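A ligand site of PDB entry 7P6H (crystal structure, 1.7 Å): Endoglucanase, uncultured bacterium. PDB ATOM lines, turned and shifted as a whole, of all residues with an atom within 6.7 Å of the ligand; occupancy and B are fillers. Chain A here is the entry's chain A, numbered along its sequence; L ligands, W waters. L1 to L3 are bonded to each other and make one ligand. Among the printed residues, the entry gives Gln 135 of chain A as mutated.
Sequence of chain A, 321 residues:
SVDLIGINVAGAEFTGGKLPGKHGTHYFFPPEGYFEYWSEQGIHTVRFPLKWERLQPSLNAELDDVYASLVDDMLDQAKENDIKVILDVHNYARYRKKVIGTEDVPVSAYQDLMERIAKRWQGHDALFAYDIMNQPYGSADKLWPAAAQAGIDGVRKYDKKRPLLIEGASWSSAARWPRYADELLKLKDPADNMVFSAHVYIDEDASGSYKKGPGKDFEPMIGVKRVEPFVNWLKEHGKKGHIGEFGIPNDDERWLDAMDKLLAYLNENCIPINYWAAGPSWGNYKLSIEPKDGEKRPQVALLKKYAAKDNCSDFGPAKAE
O3 of LG3 L3 lies within hydrogen-bond range of OE1 of Gln 135, at 2.6 Å. The backbone carbonyl oxygen (O) of Asp 205 is in hydrogen-bond range of an oxygen (O1) of LG2 L2, at 2.7 Å. An oxygen (O5) of LG3 L3 lies within hydrogen-bond range of the backbone carbonyl oxygen (O) of Ala 206. The guanidinium group of Arg 176 sits at hydrogen-bond distance from an oxygen (O1) of LG2 L2 (3.0 Å).
The side-chain amide nitrogen (NE2) of Gln 135 sits at hydrogen-bond distance from the side-chain carboxylate (OE1) of Glu 245, at 3.4 Å. NE2 of Gln 135 lies within hydrogen-bond range of ND1 of His 199 (2.9 Å). The side-chain hydroxyl (OG) of Ser 207 sits at hydrogen-bond distance from the side-chain carboxylate (OD1) of Asp 205 (2.7 Å). OG of Ser 170 lies within hydrogen-bond range of NE of Arg 176. N of Arg 176 is in hydrogen-bond range of OG of Ser 173. The side-chain hydroxyl of Ser 207 lies within hydrogen-bond range of the side-chain hydroxyl of Ser 209, at 3.1 Å. OH of Tyr 201 is in hydrogen-bond range of OE1 of Glu 245 (2.6 Å). O of Tyr 201 sits at hydrogen-bond distance from NH1 of Arg 226 (2.9 Å).
NE1 of Trp 171 touches C6 of LG3 L3 (3.7 Å). Tyr 201 touches the ligand. CA of Ser 207 touches O4 of LG3 L3, 3.3 Å away. Seven residues have an atom within 4 Å of the ligand: Gln 135, Trp 171, Arg 176, Tyr 201, Asp 205, Ala 206 and Ser 207. The nearest printed residue that does not touch the ligand is Glu 204 (4.7 Å).
Water W4 bridges O2 of LG3 L3 and OH of Tyr 92. Water W2 lies within hydrogen-bond range of O6 of LIG L1, O of Glu 204 and NH2 of Arg 226. Water W6 lies within hydrogen-bond range of O2 of LG2 L2 (2.7 Å) and NH2 of Arg 176 (3.0 Å). Water W1 lies within hydrogen-bond range of O of Trp 171 (2.8 Å) and O5 of LG3 L3 (2.8 Å). Water W3 lies within hydrogen-bond range of the indole nitrogen (NE1) of Trp 171 and an oxygen (O1) of LG3 L3.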
ATOM      1  N   TYR A  92      -5.741 -11.433 -21.481  1.00  0.00           N
ATOM      2  CA  TYR A  92      -5.014 -11.123 -22.704  1.00  0.00           C
ATOM      3  C   TYR A  92      -5.742 -10.072 -23.539  1.00  0.00           C
ATOM      4  O   TYR A  92      -5.656 -10.071 -24.763  1.00  0.00           O
ATOM      5  CB  TYR A  92      -4.762 -12.388 -23.533  1.00  0.00           C
ATOM      6  CG  TYR A  92      -4.230 -13.519 -22.685  1.00  0.00           C
ATOM      7  CD1 TYR A  92      -2.873 -13.633 -22.437  1.00  0.00           C
ATOM      8  CD2 TYR A  92      -5.076 -14.461 -22.112  1.00  0.00           C
ATOM      9  CE1 TYR A  92      -2.364 -14.661 -21.652  1.00  0.00           C
ATOM     10  CE2 TYR A  92      -4.578 -15.514 -21.317  1.00  0.00           C
ATOM     11  CZ  TYR A  92      -3.209 -15.590 -21.107  1.00  0.00           C
ATOM     12  OH  TYR A  92      -2.675 -16.585 -20.331  1.00  0.00           O
ATOM     13  N   ASN A 134      -4.178  -9.289 -17.664  1.00  0.00           N
ATOM     14  CA  ASN A 134      -2.991 -10.093 -17.879  1.00  0.00           C
ATOM     15  C   ASN A 134      -2.610 -10.109 -19.355  1.00  0.00           C
ATOM     16  O   ASN A 134      -3.445 -10.416 -20.211  1.00  0.00           O
ATOM     17  CB  ASN A 134      -3.232 -11.541 -17.426  1.00  0.00           C
ATOM     18  CG  ASN A 134      -2.023 -12.415 -17.648  1.00  0.00           C
ATOM     19  OD1 ASN A 134      -1.010 -12.231 -16.986  1.00  0.00           O
ATOM     20  ND2 ASN A 134      -2.112 -13.356 -18.583  1.00  0.00           N
ATOM     21  N   GLN A 135      -1.342  -9.783 -19.651  1.00  0.00           N
ATOM     22  CA  GLN A 135      -0.701  -9.982 -20.952  1.00  0.00           C
ATOM     23  C   GLN A 135      -1.547  -9.634 -22.175  1.00  0.00           C
ATOM     24  O   GLN A 135      -1.859 -10.512 -22.982  1.00  0.00           O
ATOM     25  CB  GLN A 135      -0.244 -11.444 -21.044  1.00  0.00           C
ATOM     26  CG  GLN A 135       0.856 -11.766 -20.028  1.00  0.00           C
ATOM     27  CD  GLN A 135       1.495 -13.130 -20.258  1.00  0.00           C
ATOM     28  OE1 GLN A 135       1.126 -13.904 -21.162  1.00  0.00           O
ATOM     29  NE2 GLN A 135       2.489 -13.440 -19.432  1.00  0.00           N
ATOM     30  N   TYR A 137      -1.627  -8.845 -25.952  1.00  0.00           N
ATOM     31  CA  TYR A 137      -0.671  -9.222 -26.996  1.00  0.00           C
ATOM     32  C   TYR A 137      -1.329  -9.179 -28.366  1.00  0.00           C
ATOM     33  O   TYR A 137      -2.554  -9.219 -28.493  1.00  0.00           O
ATOM     34  CB  TYR A 137      -0.079 -10.630 -26.767  1.00  0.00           C
ATOM     35  CG  TYR A 137      -1.055 -11.747 -27.104  1.00  0.00           C
ATOM     36  CD1 TYR A 137      -1.174 -12.220 -28.408  1.00  0.00           C
ATOM     37  CD2 TYR A 137      -1.866 -12.309 -26.121  1.00  0.00           C
ATOM     38  CE1 TYR A 137      -2.074 -13.227 -28.726  1.00  0.00           C
ATOM     39  CE2 TYR A 137      -2.758 -13.313 -26.424  1.00  0.00           C
ATOM     40  CZ  TYR A 137      -2.850 -13.776 -27.735  1.00  0.00           C
ATOM     41  OH  TYR A 137      -3.736 -14.769 -28.043  1.00  0.00           O
ATOM     42  N   SER A 170       2.472  -6.741 -25.790  1.00  0.00           N
ATOM     43  CA  SER A 170       3.488  -7.756 -26.081  1.00  0.00           C
ATOM     44  C   SER A 170       3.721  -8.656 -24.863  1.00  0.00           C
ATOM     45  O   SER A 170       4.851  -8.839 -24.402  1.00  0.00           O
ATOM     46  CB  SER A 170       4.793  -7.089 -26.560  1.00  0.00           C
ATOM     47  OG  SER A 170       5.674  -8.025 -27.165  1.00  0.00           O
ATOM     48  N   TRP A 171       2.621  -9.181 -24.321  1.00  0.00           N
ATOM     49  CA  TRP A 171       2.642 -10.069 -23.153  1.00  0.00           C
ATOM     50  C   TRP A 171       3.287  -9.379 -21.935  1.00  0.00           C
ATOM     51  O   TRP A 171       3.928 -10.008 -21.096  1.00  0.00           O
ATOM     52  CB  TRP A 171       3.332 -11.422 -23.473  1.00  0.00           C
ATOM     53  CG  TRP A 171       2.688 -12.206 -24.613  1.00  0.00           C
ATOM     54  CD1 TRP A 171       1.637 -13.089 -24.519  1.00  0.00           C
ATOM     55  CD2 TRP A 171       3.062 -12.191 -25.988  1.00  0.00           C
ATOM     56  NE1 TRP A 171       1.331 -13.602 -25.755  1.00  0.00           N
ATOM     57  CE2 TRP A 171       2.202 -13.070 -26.679  1.00  0.00           C
ATOM     58  CE3 TRP A 171       4.047 -11.509 -26.711  1.00  0.00           C
ATOM     59  CZ2 TRP A 171       2.288 -13.282 -28.046  1.00  0.00           C
ATOM     60  CZ3 TRP A 171       4.137 -11.718 -28.087  1.00  0.00           C
ATOM     61  CH2 TRP A 171       3.270 -12.609 -28.727  1.00  0.00           C
ATOM     62  N   SER A 173       5.886  -7.726 -21.775  1.00  0.00           N
ATOM     63  CA  SER A 173       7.304  -8.027 -21.773  1.00  0.00           C
ATOM     64  C   SER A 173       8.088  -6.938 -21.065  1.00  0.00           C
ATOM     65  O   SER A 173       7.993  -5.757 -21.430  1.00  0.00           O
ATOM     66  CB  SER A 173       7.817  -8.169 -23.209  1.00  0.00           C
ATOM     67  OG  SER A 173       9.233  -8.077 -23.270  1.00  0.00           O
ATOM     68  N   ARG A 176      10.944  -5.866 -23.701  1.00  0.00           N
ATOM     69  CA  ARG A 176      10.545  -4.994 -24.792  1.00  0.00           C
ATOM     70  C   ARG A 176       9.755  -3.786 -24.294  1.00  0.00           C
ATOM     71  O   ARG A 176       9.260  -2.990 -25.098  1.00  0.00           O
ATOM     72  CB  ARG A 176       9.707  -5.778 -25.828  1.00  0.00           C
ATOM     73  CG  ARG A 176      10.462  -6.941 -26.496  1.00  0.00           C
ATOM     74  CD  ARG A 176       9.596  -7.626 -27.586  1.00  0.00           C
ATOM     75  NE  ARG A 176       8.424  -8.282 -27.023  1.00  0.00           N
ATOM     76  CZ  ARG A 176       8.428  -9.520 -26.523  1.00  0.00           C
ATOM     77  NH1 ARG A 176       9.541 -10.237 -26.491  1.00  0.00           N
ATOM     78  NH2 ARG A 176       7.306 -10.033 -26.044  1.00  0.00           N
ATOM     79  N   ARG A 179       9.599  -0.281 -25.883  1.00  0.00           N
ATOM     80  CA  ARG A 179       9.190  -0.201 -27.272  1.00  0.00           C
ATOM     81  C   ARG A 179       7.757   0.261 -27.413  1.00  0.00           C
ATOM     82  O   ARG A 179       7.403   0.881 -28.424  1.00  0.00           O
ATOM     83  CB  ARG A 179       9.361  -1.552 -27.960  1.00  0.00           C
ATOM     84  CG  ARG A 179      10.763  -2.089 -27.955  1.00  0.00           C
ATOM     85  CD  ARG A 179      10.828  -3.323 -28.861  1.00  0.00           C
ATOM     86  NE  ARG A 179      12.053  -4.073 -28.645  1.00  0.00           N
ATOM     87  CZ  ARG A 179      12.290  -5.276 -29.154  1.00  0.00           C
ATOM     88  NH1 ARG A 179      11.399  -5.871 -29.929  1.00  0.00           N
ATOM     89  NH2 ARG A 179      13.429  -5.897 -28.865  1.00  0.00           N
ATOM     90  N   HIS A 199       6.344  -8.681 -17.142  1.00  0.00           N
ATOM     91  CA  HIS A 199       6.622 -10.104 -16.981  1.00  0.00           C
ATOM     92  C   HIS A 199       7.992 -10.466 -17.579  1.00  0.00           C
ATOM     93  O   HIS A 199       8.476  -9.835 -18.522  1.00  0.00           O
ATOM     94  CB  HIS A 199       5.514 -10.959 -17.617  1.00  0.00           C
ATOM     95  CG  HIS A 199       4.168 -10.780 -16.979  1.00  0.00           C
ATOM     96  ND1 HIS A 199       3.056 -11.488 -17.383  1.00  0.00           N
ATOM     97  CD2 HIS A 199       3.759  -9.962 -15.979  1.00  0.00           C
ATOM     98  CE1 HIS A 199       2.016 -11.135 -16.650  1.00  0.00           C
ATOM     99  NE2 HIS A 199       2.412 -10.176 -15.811  1.00  0.00           N
ATOM    100  N   VAL A 200       8.630 -11.477 -16.998  1.00  0.00           N
ATOM    101  CA  VAL A 200       9.933 -11.901 -17.509  1.00  0.00           C
ATOM    102  C   VAL A 200      10.125 -13.404 -17.336  1.00  0.00           C
ATOM    103  O   VAL A 200       9.986 -13.954 -16.238  1.00  0.00           O
ATOM    104  CB  VAL A 200      11.085 -11.122 -16.851  1.00  0.00           C
ATOM    105  CG1 VAL A 200      11.040 -11.207 -15.331  1.00  0.00           C
ATOM    106  CG2 VAL A 200      12.415 -11.635 -17.376  1.00  0.00           C
ATOM    107  N   TYR A 201      10.388 -14.078 -18.455  1.00  0.00           N
ATOM    108  CA  TYR A 201      10.831 -15.463 -18.487  1.00  0.00           C
ATOM    109  C   TYR A 201      12.179 -15.492 -19.180  1.00  0.00           C
ATOM    110  O   TYR A 201      12.481 -14.628 -20.014  1.00  0.00           O
ATOM    111  CB  TYR A 201       9.818 -16.347 -19.221  1.00  0.00           C
ATOM    112  CG  TYR A 201       8.523 -16.483 -18.444  1.00  0.00           C
ATOM    113  CD1 TYR A 201       8.392 -17.433 -17.434  1.00  0.00           C
ATOM    114  CD2 TYR A 201       7.461 -15.614 -18.671  1.00  0.00           C
ATOM    115  CE1 TYR A 201       7.235 -17.560 -16.711  1.00  0.00           C
ATOM    116  CE2 TYR A 201       6.264 -15.732 -17.950  1.00  0.00           C
ATOM    117  CZ  TYR A 201       6.168 -16.699 -16.966  1.00  0.00           C
ATOM    118  OH  TYR A 201       4.987 -16.832 -16.244  1.00  0.00           O
ATOM    119  N   GLU A 204      14.890 -18.763 -24.146  1.00  0.00           N
ATOM    120  CA  GLU A 204      15.381 -17.922 -25.245  1.00  0.00           C
ATOM    121  C   GLU A 204      14.297 -16.975 -25.762  1.00  0.00           C
ATOM    122  O   GLU A 204      14.524 -15.767 -25.877  1.00  0.00           O
ATOM    123  CB  GLU A 204      15.925 -18.806 -26.376  1.00  0.00           C
ATOM    124  CG  GLU A 204      16.854 -18.067 -27.332  1.00  0.00           C
ATOM    125  CD  GLU A 204      16.110 -17.063 -28.203  1.00  0.00           C
ATOM    126  OE1 GLU A 204      15.081 -17.459 -28.794  1.00  0.00           O
ATOM    127  OE2 GLU A 204      16.536 -15.881 -28.279  1.00  0.00           O
ATOM    128  N   ASP A 205      13.108 -17.495 -26.055  1.00  0.00           N
ATOM    129  CA  ASP A 205      12.056 -16.649 -26.610  1.00  0.00           C
ATOM    130  C   ASP A 205      11.178 -16.001 -25.552  1.00  0.00           C
ATOM    131  O   ASP A 205      10.172 -15.364 -25.906  1.00  0.00           O
ATOM    132  CB  ASP A 205      11.191 -17.447 -27.606  1.00  0.00           C
ATOM    133  CG  ASP A 205      10.299 -18.487 -26.952  1.00  0.00           C
ATOM    134  OD1 ASP A 205      10.313 -18.664 -25.710  1.00  0.00           O
ATOM    135  OD2 ASP A 205       9.558 -19.143 -27.711  1.00  0.00           O
ATOM    136  N   ALA A 206      11.518 -16.143 -24.263  1.00  0.00           N
ATOM    137  CA  ALA A 206      10.832 -15.494 -23.147  1.00  0.00           C
ATOM    138  C   ALA A 206       9.365 -15.889 -23.044  1.00  0.00           C
ATOM    139  O   ALA A 206       8.559 -15.176 -22.428  1.00  0.00           O
ATOM    140  CB  ALA A 206      10.971 -13.958 -23.249  1.00  0.00           C
ATOM    141  N   SER A 207       8.987 -17.032 -23.627  1.00  0.00           N
ATOM    142  CA  SER A 207       7.622 -17.534 -23.511  1.00  0.00           C
ATOM    143  C   SER A 207       7.371 -18.267 -22.199  1.00  0.00           C
ATOM    144  O   SER A 207       6.214 -18.565 -21.915  1.00  0.00           O
ATOM    145  CB  SER A 207       7.298 -18.479 -24.662  1.00  0.00           C
ATOM    146  OG  SER A 207       8.084 -19.647 -24.521  1.00  0.00           O
ATOM    147  N   GLY A 208       8.414 -18.580 -21.434  1.00  0.00           N
ATOM    148  CA  GLY A 208       8.234 -19.409 -20.257  1.00  0.00           C
ATOM    149  C   GLY A 208       7.900 -20.851 -20.547  1.00  0.00           C
ATOM    150  O   GLY A 208       7.444 -21.567 -19.649  1.00  0.00           O
ATOM    151  N   SER A 209       8.126 -21.314 -21.782  1.00  0.00           N
ATOM    152  CA  SER A 209       7.877 -22.700 -22.152  1.00  0.00           C
ATOM    153  C   SER A 209       8.992 -23.629 -21.684  1.00  0.00           C
ATOM    154  O   SER A 209       8.738 -24.803 -21.394  1.00  0.00           O
ATOM    155  CB  SER A 209       7.728 -22.794 -23.663  1.00  0.00           C
ATOM    156  OG  SER A 209       6.490 -22.281 -24.083  1.00  0.00           O
ATOM    157  N   ARG A 226      16.935  -8.536 -18.881  1.00  0.00           N
ATOM    158  CA  ARG A 226      15.594  -8.442 -19.443  1.00  0.00           C
ATOM    159  C   ARG A 226      14.672  -7.533 -18.647  1.00  0.00           C
ATOM    160  O   ARG A 226      13.686  -7.045 -19.213  1.00  0.00           O
ATOM    161  CB  ARG A 226      14.982  -9.840 -19.589  1.00  0.00           C
ATOM    162  CG  ARG A 226      15.488 -10.522 -20.840  1.00  0.00           C
ATOM    163  CD  ARG A 226      14.918 -11.930 -21.030  1.00  0.00           C
ATOM    164  NE  ARG A 226      15.533 -12.502 -22.226  1.00  0.00           N
ATOM    165  CZ  ARG A 226      15.162 -13.643 -22.793  1.00  0.00           C
ATOM    166  NH1 ARG A 226      14.194 -14.384 -22.282  1.00  0.00           N
ATOM    167  NH2 ARG A 226      15.776 -14.045 -23.898  1.00  0.00           N
ATOM    168  N   GLU A 245       4.958 -11.756 -13.232  1.00  0.00           N
ATOM    169  CA  GLU A 245       5.236 -13.162 -13.550  1.00  0.00           C
ATOM    170  C   GLU A 245       6.726 -13.361 -13.835  1.00  0.00           C
ATOM    171  O   GLU A 245       7.324 -12.594 -14.594  1.00  0.00           O
ATOM    172  CB  GLU A 245       4.461 -13.636 -14.783  1.00  0.00           C
ATOM    173  CG  GLU A 245       2.971 -13.797 -14.549  1.00  0.00           C
ATOM    174  CD  GLU A 245       2.272 -14.482 -15.684  1.00  0.00           C
ATOM    175  OE1 GLU A 245       2.953 -15.185 -16.500  1.00  0.00           O
ATOM    176  OE2 GLU A 245       1.043 -14.330 -15.760  1.00  0.00           O
HETATM  177  C1  LIG L   1      10.732 -12.673 -32.492  1.00  0.00           C
HETATM  178  C2  LIG L   1       9.303 -13.120 -32.625  1.00  0.00           C
HETATM  179  C3  LIG L   1       8.506 -13.142 -31.385  1.00  0.00           C
HETATM  180  C4  LIG L   1       9.214 -13.528 -30.143  1.00  0.00           C
HETATM  181  C5  LIG L   1      10.642 -12.911 -30.035  1.00  0.00           C
HETATM  182  C6  LIG L   1      11.335 -13.472 -28.915  1.00  0.00           C
HETATM  183  O1  LIG L   1      10.774 -11.283 -32.393  1.00  0.00           O
HETATM  184  O2  LIG L   1       8.618 -12.188 -33.558  1.00  0.00           O
HETATM  185  O3  LIG L   1       7.400 -14.130 -31.610  1.00  0.00           O
HETATM  186  O4  LIG L   1       8.451 -13.028 -29.015  1.00  0.00           O
HETATM  187  O5  LIG L   1      11.398 -13.234 -31.315  1.00  0.00           O
HETATM  188  O6  LIG L   1      12.441 -12.611 -28.614  1.00  0.00           O
HETATM  189  C1  LG2 L   2       7.538 -13.547 -26.889  1.00  0.00           C
HETATM  190  C2  LG2 L   2       6.833 -14.532 -26.054  1.00  0.00           C
HETATM  191  C3  LG2 L   2       5.631 -15.115 -26.724  1.00  0.00           C
HETATM  192  C4  LG2 L   2       5.995 -15.649 -28.149  1.00  0.00           C
HETATM  193  C5  LG2 L   2       4.839 -15.988 -28.875  1.00  0.00           C
HETATM  194  C6  LG2 L   2       7.906 -14.073 -28.240  1.00  0.00           C
HETATM  195  O1  LG2 L   2       8.757 -13.102 -26.175  1.00  0.00           O
HETATM  196  O2  LG2 L   2       6.427 -13.795 -24.819  1.00  0.00           O
HETATM  197  O3  LG2 L   2       5.105 -16.256 -26.014  1.00  0.00           O
HETATM  198  O4  LG2 L   2       6.715 -14.546 -28.931  1.00  0.00           O
HETATM  199  O5  LG2 L   2       5.291 -16.547 -30.100  1.00  0.00           O
HETATM  200  C1  LG3 L   3       3.197 -17.070 -24.865  1.00  0.00           C
HETATM  201  C2  LG3 L   3       2.304 -16.833 -23.747  1.00  0.00           C
HETATM  202  C3  LG3 L   3       3.059 -16.583 -22.484  1.00  0.00           C
HETATM  203  C4  LG3 L   3       4.066 -15.406 -22.607  1.00  0.00           C
HETATM  204  C5  LG3 L   3       4.957 -15.335 -21.498  1.00  0.00           C
HETATM  205  C6  LG3 L   3       4.144 -15.930 -25.051  1.00  0.00           C
HETATM  206  O1  LG3 L   3       2.442 -17.254 -26.124  1.00  0.00           O
HETATM  207  O2  LG3 L   3       1.405 -17.999 -23.528  1.00  0.00           O
HETATM  208  O3  LG3 L   3       2.135 -16.311 -21.446  1.00  0.00           O
HETATM  209  O4  LG3 L   3       4.903 -15.705 -23.832  1.00  0.00           O
HETATM  210  O5  LG3 L   3       5.953 -14.358 -21.787  1.00  0.00           O
HETATM  211  O   HOH W   1       6.205 -11.573 -21.249  1.00  0.00           O
HETATM  212  O   HOH W   2      13.480 -13.236 -26.322  1.00  0.00           O
HETATM  213  O   HOH W   3      -0.162 -15.976 -26.593  1.00  0.00           O
HETATM  214  O   HOH W   4      -0.647 -18.012 -22.176  1.00  0.00           O
HETATM  215  O   HOH W   5       3.058 -19.261 -27.627  1.00  0.00           O
HETATM  216  O   HOH W   6       7.764 -11.697 -23.649  1.00  0.00           O
